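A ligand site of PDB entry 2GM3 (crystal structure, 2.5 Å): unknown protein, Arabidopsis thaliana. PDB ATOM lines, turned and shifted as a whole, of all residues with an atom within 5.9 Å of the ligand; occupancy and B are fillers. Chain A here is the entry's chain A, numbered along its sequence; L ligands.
A nitrogen (N4) of the ligand sits close to the backbone carbonyl oxygen (O) of Val 12 (3.3 Å).
Merely in contact with the ligand: Asn 13 (3.3 Å), Leu 51 (3.6 Å), His 52 (3.9 Å), Pro 112 (3.6 Å), Ile 116 (3.7 Å), Val 130 (3.4 Å), Ser 132 (3.7 Å) and Thr 145 (3.7 Å).
Of the 27 residues printed, 17 come within 4 Å of the ligand.
The nearest printed residue that does not touch the ligand is Ser 24 (4.02 Å).
The side-chain hydroxyl (OG) of Ser 26 is in hydrogen-bond range of the side-chain carboxylate (OD1) of Asp 175.
NH2 of Arg 133 sits at hydrogen-bond distance from OG1 of Thr 145, 3.4 Å away.
N of Val 12 is in hydrogen-bond range of O of Leu 51 (2.9 Å).
The backbone carbonyl oxygen of Val 12 lies within hydrogen-bond range of a ring nitrogen (ND1) of His 52 (2.9 Å).
The backbone NH (N) of Asn 13 is in hydrogen-bond range of the side-chain sulfur (SG) of Cys 27, 3.5 Å away.
N of Cys 27 sits at hydrogen-bond distance from OG of Ser 24 (3.2 Å).
N of Leu 51 is in hydrogen-bond range of O of Val 10.
The side-chain hydroxyl of Ser 132 is in hydrogen-bond range of the backbone NH of Gly 134, 3.0 Å away.
N of Ser 147 sits at hydrogen-bond distance from O3 of the ligand.
An oxygen (O3) of the ligand lies within hydrogen-bond range of the side-chain hydroxyl of Ser 147 (2.5 Å).
The backbone carbonyl oxygen (O) of Ala 11 is in hydrogen-bond range of an oxygen (O7) of the ligand.
The side-chain hydroxyl (OG) of Ser 26 sits at hydrogen-bond distance from an oxygen (O6) of the ligand (2.7 Å).
The backbone NH (N) of Arg 133 sits at hydrogen-bond distance from an oxygen (O2) of the ligand.
O2 of the ligand is in salt-bridge range of NE of Arg 133 (2.7 Å).
N of Val 53 is in hydrogen-bond range of N4 of the ligand (2.9 Å).
N3 of the ligand sits at hydrogen-bond distance from O of Val 53 (2.8 Å).
The backbone NH (N) of Gly 131 is in hydrogen-bond range of an oxygen (O7) of the ligand, at 3.0 Å.
The backbone NH of Cys 27 is in hydrogen-bond range of an oxygen (O6) of the ligand, 3.3 Å away.
An oxygen (O1) of the ligand lies within hydrogen-bond range of the backbone NH (N) of Val 146 (3.3 Å).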
ATOM      1  N   VAL A  10     -13.321 -22.644  -1.979  1.00  0.00           N
ATOM      2  CA  VAL A  10     -14.669 -22.122  -1.673  1.00  0.00           C
ATOM      3  C   VAL A  10     -15.030 -21.166  -2.788  1.00  0.00           C
ATOM      4  O   VAL A  10     -14.358 -20.187  -2.986  1.00  0.00           O
ATOM      5  CB  VAL A  10     -14.714 -21.394  -0.335  1.00  0.00           C
ATOM      6  CG1 VAL A  10     -16.102 -20.869  -0.088  1.00  0.00           C
ATOM      7  CG2 VAL A  10     -14.295 -22.315   0.816  1.00  0.00           C
ATOM      8  N   ALA A  11     -16.086 -21.491  -3.525  1.00  0.00           N
ATOM      9  CA  ALA A  11     -16.486 -20.728  -4.675  1.00  0.00           C
ATOM     10  C   ALA A  11     -17.441 -19.640  -4.159  1.00  0.00           C
ATOM     11  O   ALA A  11     -18.505 -19.953  -3.618  1.00  0.00           O
ATOM     12  CB  ALA A  11     -17.186 -21.647  -5.661  1.00  0.00           C
ATOM     13  N   VAL A  12     -17.054 -18.382  -4.338  1.00  0.00           N
ATOM     14  CA  VAL A  12     -17.823 -17.257  -3.779  1.00  0.00           C
ATOM     15  C   VAL A  12     -18.291 -16.323  -4.874  1.00  0.00           C
ATOM     16  O   VAL A  12     -17.578 -16.058  -5.867  1.00  0.00           O
ATOM     17  CB  VAL A  12     -17.027 -16.475  -2.688  1.00  0.00           C
ATOM     18  CG1 VAL A  12     -16.584 -17.414  -1.534  1.00  0.00           C
ATOM     19  CG2 VAL A  12     -15.828 -15.783  -3.257  1.00  0.00           C
ATOM     20  N   ASN A  13     -19.518 -15.834  -4.721  1.00  0.00           N
ATOM     21  CA  ASN A  13     -20.080 -14.898  -5.666  1.00  0.00           C
ATOM     22  C   ASN A  13     -20.881 -13.804  -4.965  1.00  0.00           C
ATOM     23  O   ASN A  13     -21.119 -13.877  -3.742  1.00  0.00           O
ATOM     24  CB  ASN A  13     -20.941 -15.633  -6.679  1.00  0.00           C
ATOM     25  CG  ASN A  13     -22.135 -16.288  -6.038  1.00  0.00           C
ATOM     26  OD1 ASN A  13     -22.045 -16.924  -4.962  1.00  0.00           O
ATOM     27  ND2 ASN A  13     -23.275 -16.152  -6.689  1.00  0.00           N
ATOM     28  N   SER A  24     -23.187 -13.575  -1.985  1.00  0.00           N
ATOM     29  CA  SER A  24     -24.492 -14.245  -2.075  1.00  0.00           C
ATOM     30  C   SER A  24     -24.789 -14.932  -0.745  1.00  0.00           C
ATOM     31  O   SER A  24     -23.861 -15.393  -0.054  1.00  0.00           O
ATOM     32  CB  SER A  24     -24.482 -15.256  -3.231  1.00  0.00           C
ATOM     33  OG  SER A  24     -23.744 -16.431  -2.932  1.00  0.00           O
ATOM     34  N   SER A  26     -25.939 -17.785  -0.317  1.00  0.00           N
ATOM     35  CA  SER A  26     -25.602 -19.186  -0.328  1.00  0.00           C
ATOM     36  C   SER A  26     -24.109 -19.447  -0.093  1.00  0.00           C
ATOM     37  O   SER A  26     -23.720 -20.347   0.666  1.00  0.00           O
ATOM     38  CB  SER A  26     -26.145 -19.864  -1.604  1.00  0.00           C
ATOM     39  OG  SER A  26     -25.437 -19.432  -2.736  1.00  0.00           O
ATOM     40  N   CYS A  27     -23.258 -18.661  -0.722  1.00  0.00           N
ATOM     41  CA  CYS A  27     -21.833 -18.917  -0.596  1.00  0.00           C
ATOM     42  C   CYS A  27     -21.379 -18.409   0.755  1.00  0.00           C
ATOM     43  O   CYS A  27     -20.424 -18.927   1.305  1.00  0.00           O
ATOM     44  CB  CYS A  27     -21.021 -18.295  -1.734  1.00  0.00           C
ATOM     45  SG  CYS A  27     -20.663 -16.517  -1.528  1.00  0.00           S
ATOM     46  N   LYS A  28     -22.073 -17.451   1.316  1.00  0.00           N
ATOM     47  CA  LYS A  28     -21.757 -16.952   2.626  1.00  0.00           C
ATOM     48  C   LYS A  28     -22.086 -18.024   3.647  1.00  0.00           C
ATOM     49  O   LYS A  28     -21.265 -18.337   4.547  1.00  0.00           O
ATOM     50  CB  LYS A  28     -22.578 -15.693   2.915  1.00  0.00           C
ATOM     51  CG  LYS A  28     -22.008 -14.836   4.049  1.00  0.00           C
ATOM     52  CD  LYS A  28     -22.874 -13.586   4.348  1.00  0.00           C
ATOM     53  CE  LYS A  28     -22.622 -13.117   5.770  1.00  0.00           C
ATOM     54  NZ  LYS A  28     -23.219 -11.763   6.042  1.00  0.00           N
ATOM     55  N   ALA A  30     -22.384 -21.136   2.979  1.00  0.00           N
ATOM     56  CA  ALA A  30     -21.447 -22.208   2.676  1.00  0.00           C
ATOM     57  C   ALA A  30     -20.084 -22.021   3.367  1.00  0.00           C
ATOM     58  O   ALA A  30     -19.548 -22.957   3.960  1.00  0.00           O
ATOM     59  CB  ALA A  30     -21.261 -22.304   1.197  1.00  0.00           C
ATOM     60  N   LEU A  51     -12.222 -18.673  -4.508  1.00  0.00           N
ATOM     61  CA  LEU A  51     -12.276 -18.351  -5.906  1.00  0.00           C
ATOM     62  C   LEU A  51     -13.573 -17.633  -6.271  1.00  0.00           C
ATOM     63  O   LEU A  51     -14.686 -18.124  -5.962  1.00  0.00           O
ATOM     64  CB  LEU A  51     -12.097 -19.610  -6.728  1.00  0.00           C
ATOM     65  CG  LEU A  51     -12.485 -19.497  -8.202  1.00  0.00           C
ATOM     66  CD1 LEU A  51     -11.477 -18.724  -9.031  1.00  0.00           C
ATOM     67  CD2 LEU A  51     -12.656 -20.905  -8.751  1.00  0.00           C
ATOM     68  N   HIS A  52     -13.432 -16.495  -6.945  1.00  0.00           N
ATOM     69  CA  HIS A  52     -14.560 -15.800  -7.556  1.00  0.00           C
ATOM     70  C   HIS A  52     -14.439 -15.865  -9.041  1.00  0.00           C
ATOM     71  O   HIS A  52     -13.395 -15.532  -9.607  1.00  0.00           O
ATOM     72  CB  HIS A  52     -14.615 -14.331  -7.134  1.00  0.00           C
ATOM     73  CG  HIS A  52     -15.688 -13.579  -7.836  1.00  0.00           C
ATOM     74  ND1 HIS A  52     -17.033 -13.804  -7.599  1.00  0.00           N
ATOM     75  CD2 HIS A  52     -15.636 -12.590  -8.762  1.00  0.00           C
ATOM     76  CE1 HIS A  52     -17.752 -12.989  -8.341  1.00  0.00           C
ATOM     77  NE2 HIS A  52     -16.933 -12.229  -9.053  1.00  0.00           N
ATOM     78  N   VAL A  53     -15.495 -16.293  -9.708  1.00  0.00           N
ATOM     79  CA  VAL A  53     -15.485 -16.231 -11.159  1.00  0.00           C
ATOM     80  C   VAL A  53     -16.228 -14.994 -11.628  1.00  0.00           C
ATOM     81  O   VAL A  53     -17.375 -14.787 -11.307  1.00  0.00           O
ATOM     82  CB  VAL A  53     -15.986 -17.527 -11.801  1.00  0.00           C
ATOM     83  CG1 VAL A  53     -15.769 -17.519 -13.320  1.00  0.00           C
ATOM     84  CG2 VAL A  53     -15.216 -18.673 -11.219  1.00  0.00           C
ATOM     85  N   GLN A  54     -15.546 -14.174 -12.393  1.00  0.00           N
ATOM     86  CA  GLN A  54     -16.108 -12.922 -12.908  1.00  0.00           C
ATOM     87  C   GLN A  54     -16.595 -13.072 -14.362  1.00  0.00           C
ATOM     88  O   GLN A  54     -15.925 -13.692 -15.196  1.00  0.00           O
ATOM     89  CB  GLN A  54     -15.027 -11.857 -12.792  1.00  0.00           C
ATOM     90  CG  GLN A  54     -15.423 -10.446 -13.020  1.00  0.00           C
ATOM     91  CD  GLN A  54     -14.276  -9.630 -13.627  1.00  0.00           C
ATOM     92  OE1 GLN A  54     -13.118  -9.751 -13.209  1.00  0.00           O
ATOM     93  NE2 GLN A  54     -14.613  -8.803 -14.609  1.00  0.00           N
ATOM     94  N   PRO A 112     -18.699 -19.268 -14.826  1.00  0.00           N
ATOM     95  CA  PRO A 112     -18.396 -19.716 -13.461  1.00  0.00           C
ATOM     96  C   PRO A 112     -18.306 -21.238 -13.255  1.00  0.00           C
ATOM     97  O   PRO A 112     -17.320 -21.694 -12.681  1.00  0.00           O
ATOM     98  CB  PRO A 112     -19.515 -19.089 -12.615  1.00  0.00           C
ATOM     99  CG  PRO A 112     -19.885 -17.858 -13.363  1.00  0.00           C
ATOM    100  CD  PRO A 112     -19.759 -18.249 -14.829  1.00  0.00           C
ATOM    101  N   ILE A 116     -14.727 -22.851 -12.342  1.00  0.00           N
ATOM    102  CA  ILE A 116     -14.570 -23.525 -11.051  1.00  0.00           C
ATOM    103  C   ILE A 116     -13.962 -24.904 -11.267  1.00  0.00           C
ATOM    104  O   ILE A 116     -12.998 -25.268 -10.581  1.00  0.00           O
ATOM    105  CB  ILE A 116     -15.909 -23.714 -10.303  1.00  0.00           C
ATOM    106  CG1 ILE A 116     -16.498 -22.365  -9.929  1.00  0.00           C
ATOM    107  CG2 ILE A 116     -15.731 -24.641  -9.071  1.00  0.00           C
ATOM    108  CD1 ILE A 116     -17.874 -22.480  -9.325  1.00  0.00           C
ATOM    109  N   VAL A 129     -16.064 -26.394  -1.865  1.00  0.00           N
ATOM    110  CA  VAL A 129     -17.312 -25.994  -1.220  1.00  0.00           C
ATOM    111  C   VAL A 129     -18.061 -24.995  -2.119  1.00  0.00           C
ATOM    112  O   VAL A 129     -17.497 -23.985  -2.546  1.00  0.00           O
ATOM    113  CB  VAL A 129     -17.045 -25.331   0.138  1.00  0.00           C
ATOM    114  CG1 VAL A 129     -18.341 -24.915   0.765  1.00  0.00           C
ATOM    115  CG2 VAL A 129     -16.277 -26.246   1.079  1.00  0.00           C
ATOM    116  N   VAL A 130     -19.320 -25.305  -2.406  1.00  0.00           N
ATOM    117  CA  VAL A 130     -20.184 -24.406  -3.107  1.00  0.00           C
ATOM    118  C   VAL A 130     -21.435 -24.315  -2.289  1.00  0.00           C
ATOM    119  O   VAL A 130     -21.857 -25.301  -1.672  1.00  0.00           O
ATOM    120  CB  VAL A 130     -20.522 -24.899  -4.575  1.00  0.00           C
ATOM    121  CG1 VAL A 130     -19.285 -24.840  -5.472  1.00  0.00           C
ATOM    122  CG2 VAL A 130     -21.086 -26.323  -4.567  1.00  0.00           C
ATOM    123  N   GLY A 131     -22.011 -23.116  -2.276  1.00  0.00           N
ATOM    124  CA  GLY A 131     -23.348 -22.929  -1.778  1.00  0.00           C
ATOM    125  C   GLY A 131     -24.279 -23.482  -2.833  1.00  0.00           C
ATOM    126  O   GLY A 131     -23.822 -23.910  -3.904  1.00  0.00           O
ATOM    127  N   SER A 132     -25.577 -23.500  -2.548  1.00  0.00           N
ATOM    128  CA  SER A 132     -26.555 -23.977  -3.487  1.00  0.00           C
ATOM    129  C   SER A 132     -27.893 -23.365  -3.141  1.00  0.00           C
ATOM    130  O   SER A 132     -28.249 -23.287  -1.976  1.00  0.00           O
ATOM    131  CB  SER A 132     -26.640 -25.494  -3.448  1.00  0.00           C
ATOM    132  OG  SER A 132     -27.799 -25.932  -4.149  1.00  0.00           O
ATOM    133  N   ARG A 133     -28.611 -22.918  -4.153  1.00  0.00           N
ATOM    134  CA  ARG A 133     -29.907 -22.328  -3.947  1.00  0.00           C
ATOM    135  C   ARG A 133     -30.930 -23.433  -3.890  1.00  0.00           C
ATOM    136  O   ARG A 133     -32.060 -23.192  -3.503  1.00  0.00           O
ATOM    137  CB  ARG A 133     -30.225 -21.312  -5.043  1.00  0.00           C
ATOM    138  CG  ARG A 133     -29.302 -20.099  -4.983  1.00  0.00           C
ATOM    139  CD  ARG A 133     -29.433 -19.258  -6.199  1.00  0.00           C
ATOM    140  NE  ARG A 133     -28.848 -19.917  -7.348  1.00  0.00           N
ATOM    141  CZ  ARG A 133     -28.940 -19.469  -8.612  1.00  0.00           C
ATOM    142  NH1 ARG A 133     -29.632 -18.381  -8.895  1.00  0.00           N
ATOM    143  NH2 ARG A 133     -28.336 -20.139  -9.595  1.00  0.00           N
ATOM    144  N   GLY A 134     -30.499 -24.641  -4.261  1.00  0.00           N
ATOM    145  CA  GLY A 134     -31.324 -25.835  -4.296  1.00  0.00           C
ATOM    146  C   GLY A 134     -32.388 -25.846  -5.373  1.00  0.00           C
ATOM    147  O   GLY A 134     -33.501 -26.328  -5.109  1.00  0.00           O
ATOM    148  N   LEU A 135     -32.047 -25.394  -6.565  1.00  0.00           N
ATOM    149  CA  LEU A 135     -32.981 -25.201  -7.652  1.00  0.00           C
ATOM    150  C   LEU A 135     -33.396 -26.473  -8.435  1.00  0.00           C
ATOM    151  O   LEU A 135     -33.599 -26.435  -9.650  1.00  0.00           O
ATOM    152  CB  LEU A 135     -32.420 -24.122  -8.595  1.00  0.00           C
ATOM    153  CG  LEU A 135     -32.799 -22.642  -8.390  1.00  0.00           C
ATOM    154  CD1 LEU A 135     -33.519 -22.317  -7.077  1.00  0.00           C
ATOM    155  CD2 LEU A 135     -31.521 -21.840  -8.484  1.00  0.00           C
ATOM    156  N   THR A 145     -27.927 -24.444 -11.630  1.00  0.00           N
ATOM    157  CA  THR A 145     -26.842 -24.174 -12.558  1.00  0.00           C
ATOM    158  C   THR A 145     -25.427 -24.500 -12.023  1.00  0.00           C
ATOM    159  O   THR A 145     -24.902 -25.575 -12.361  1.00  0.00           O
ATOM    160  CB  THR A 145     -26.948 -22.754 -13.278  1.00  0.00           C
ATOM    161  OG1 THR A 145     -26.955 -21.695 -12.332  1.00  0.00           O
ATOM    162  CG2 THR A 145     -28.260 -22.668 -14.135  1.00  0.00           C
ATOM    163  N   VAL A 146     -24.868 -23.657 -11.152  1.00  0.00           N
ATOM    164  CA  VAL A 146     -23.472 -23.850 -10.757  1.00  0.00           C
ATOM    165  C   VAL A 146     -23.176 -25.071  -9.880  1.00  0.00           C
ATOM    166  O   VAL A 146     -22.348 -25.916 -10.248  1.00  0.00           O
ATOM    167  CB  VAL A 146     -22.843 -22.556 -10.136  1.00  0.00           C
ATOM    168  CG1 VAL A 146     -21.383 -22.807  -9.787  1.00  0.00           C
ATOM    169  CG2 VAL A 146     -22.957 -21.392 -11.095  1.00  0.00           C
ATOM    170  N   SER A 147     -23.810 -25.149  -8.722  1.00  0.00           N
ATOM    171  CA  SER A 147     -23.509 -26.194  -7.749  1.00  0.00           C
ATOM    172  C   SER A 147     -23.716 -27.587  -8.322  1.00  0.00           C
ATOM    173  O   SER A 147     -22.910 -28.461  -8.065  1.00  0.00           O
ATOM    174  CB  SER A 147     -24.291 -26.020  -6.436  1.00  0.00           C
ATOM    175  OG  SER A 147     -25.710 -26.204  -6.617  1.00  0.00           O
ATOM    176  N   ALA A 148     -24.785 -27.797  -9.081  1.00  0.00           N
ATOM    177  CA  ALA A 148     -25.055 -29.112  -9.684  1.00  0.00           C
ATOM    178  C   ALA A 148     -23.999 -29.490 -10.721  1.00  0.00           C
ATOM    179  O   ALA A 148     -23.650 -30.645 -10.857  1.00  0.00           O
ATOM    180  CB  ALA A 148     -26.441 -29.136 -10.326  1.00  0.00           C
ATOM    181  N   ASP A 175     -30.424 -14.637  -4.683  1.00  0.00           N
ATOM    182  CA  ASP A 175     -29.264 -14.969  -3.888  1.00  0.00           C
ATOM    183  C   ASP A 175     -28.486 -13.669  -3.671  1.00  0.00           C
ATOM    184  O   ASP A 175     -27.744 -13.532  -2.675  1.00  0.00           O
ATOM    185  CB  ASP A 175     -28.410 -16.039  -4.572  1.00  0.00           C
ATOM    186  CG  ASP A 175     -27.654 -16.929  -3.600  1.00  0.00           C
ATOM    187  OD1 ASP A 175     -26.809 -17.728  -4.033  1.00  0.00           O
ATOM    188  OD2 ASP A 175     -27.883 -16.838  -2.372  1.00  0.00           O
ATOM    189  OXT ASP A 175     -28.645 -12.722  -4.482  1.00  0.00           O
HETATM  190  P1  LIG L   1     -26.324 -22.596  -7.552  1.00  0.00           P
HETATM  191  O1  LIG L   1     -26.126 -21.791  -8.710  1.00  0.00           O
HETATM  192  O2  LIG L   1     -27.383 -22.110  -6.636  1.00  0.00           O
HETATM  193  O3  LIG L   1     -26.405 -24.033  -7.743  1.00  0.00           O
HETATM  194  O4  LIG L   1     -25.023 -22.483  -6.646  1.00  0.00           O
HETATM  195  C1  LIG L   1     -24.665 -21.242  -6.073  1.00  0.00           C
HETATM  196  C2  LIG L   1     -23.205 -21.370  -5.697  1.00  0.00           C
HETATM  197  O5  LIG L   1     -22.348 -21.470  -6.880  1.00  0.00           O
HETATM  198  C3  LIG L   1     -22.700 -20.181  -4.934  1.00  0.00           C
HETATM  199  O6  LIG L   1     -23.057 -20.347  -3.536  1.00  0.00           O
HETATM  200  C4  LIG L   1     -21.196 -20.327  -5.145  1.00  0.00           C
HETATM  201  O7  LIG L   1     -20.690 -21.252  -4.187  1.00  0.00           O
HETATM  202  C5  LIG L   1     -21.089 -20.901  -6.555  1.00  0.00           C
HETATM  203  N1  LIG L   1     -21.008 -19.777  -7.507  1.00  0.00           N
HETATM  204  C6  LIG L   1     -22.005 -19.213  -8.231  1.00  0.00           C
HETATM  205  N2  LIG L   1     -21.497 -18.218  -8.971  1.00  0.00           N
HETATM  206  C7  LIG L   1     -20.185 -18.174  -8.771  1.00  0.00           C
HETATM  207  C8  LIG L   1     -19.122 -17.397  -9.256  1.00  0.00           C
HETATM  208  N3  LIG L   1     -19.292 -16.428 -10.135  1.00  0.00           N
HETATM  209  N4  LIG L   1     -17.896 -17.637  -8.801  1.00  0.00           N
HETATM  210  C9  LIG L   1     -17.643 -18.579  -7.912  1.00  0.00           C
HETATM  211  N5  LIG L   1     -18.600 -19.348  -7.430  1.00  0.00           N
HETATM  212  C10 LIG L   1     -19.874 -19.162  -7.838  1.00  0.00           C
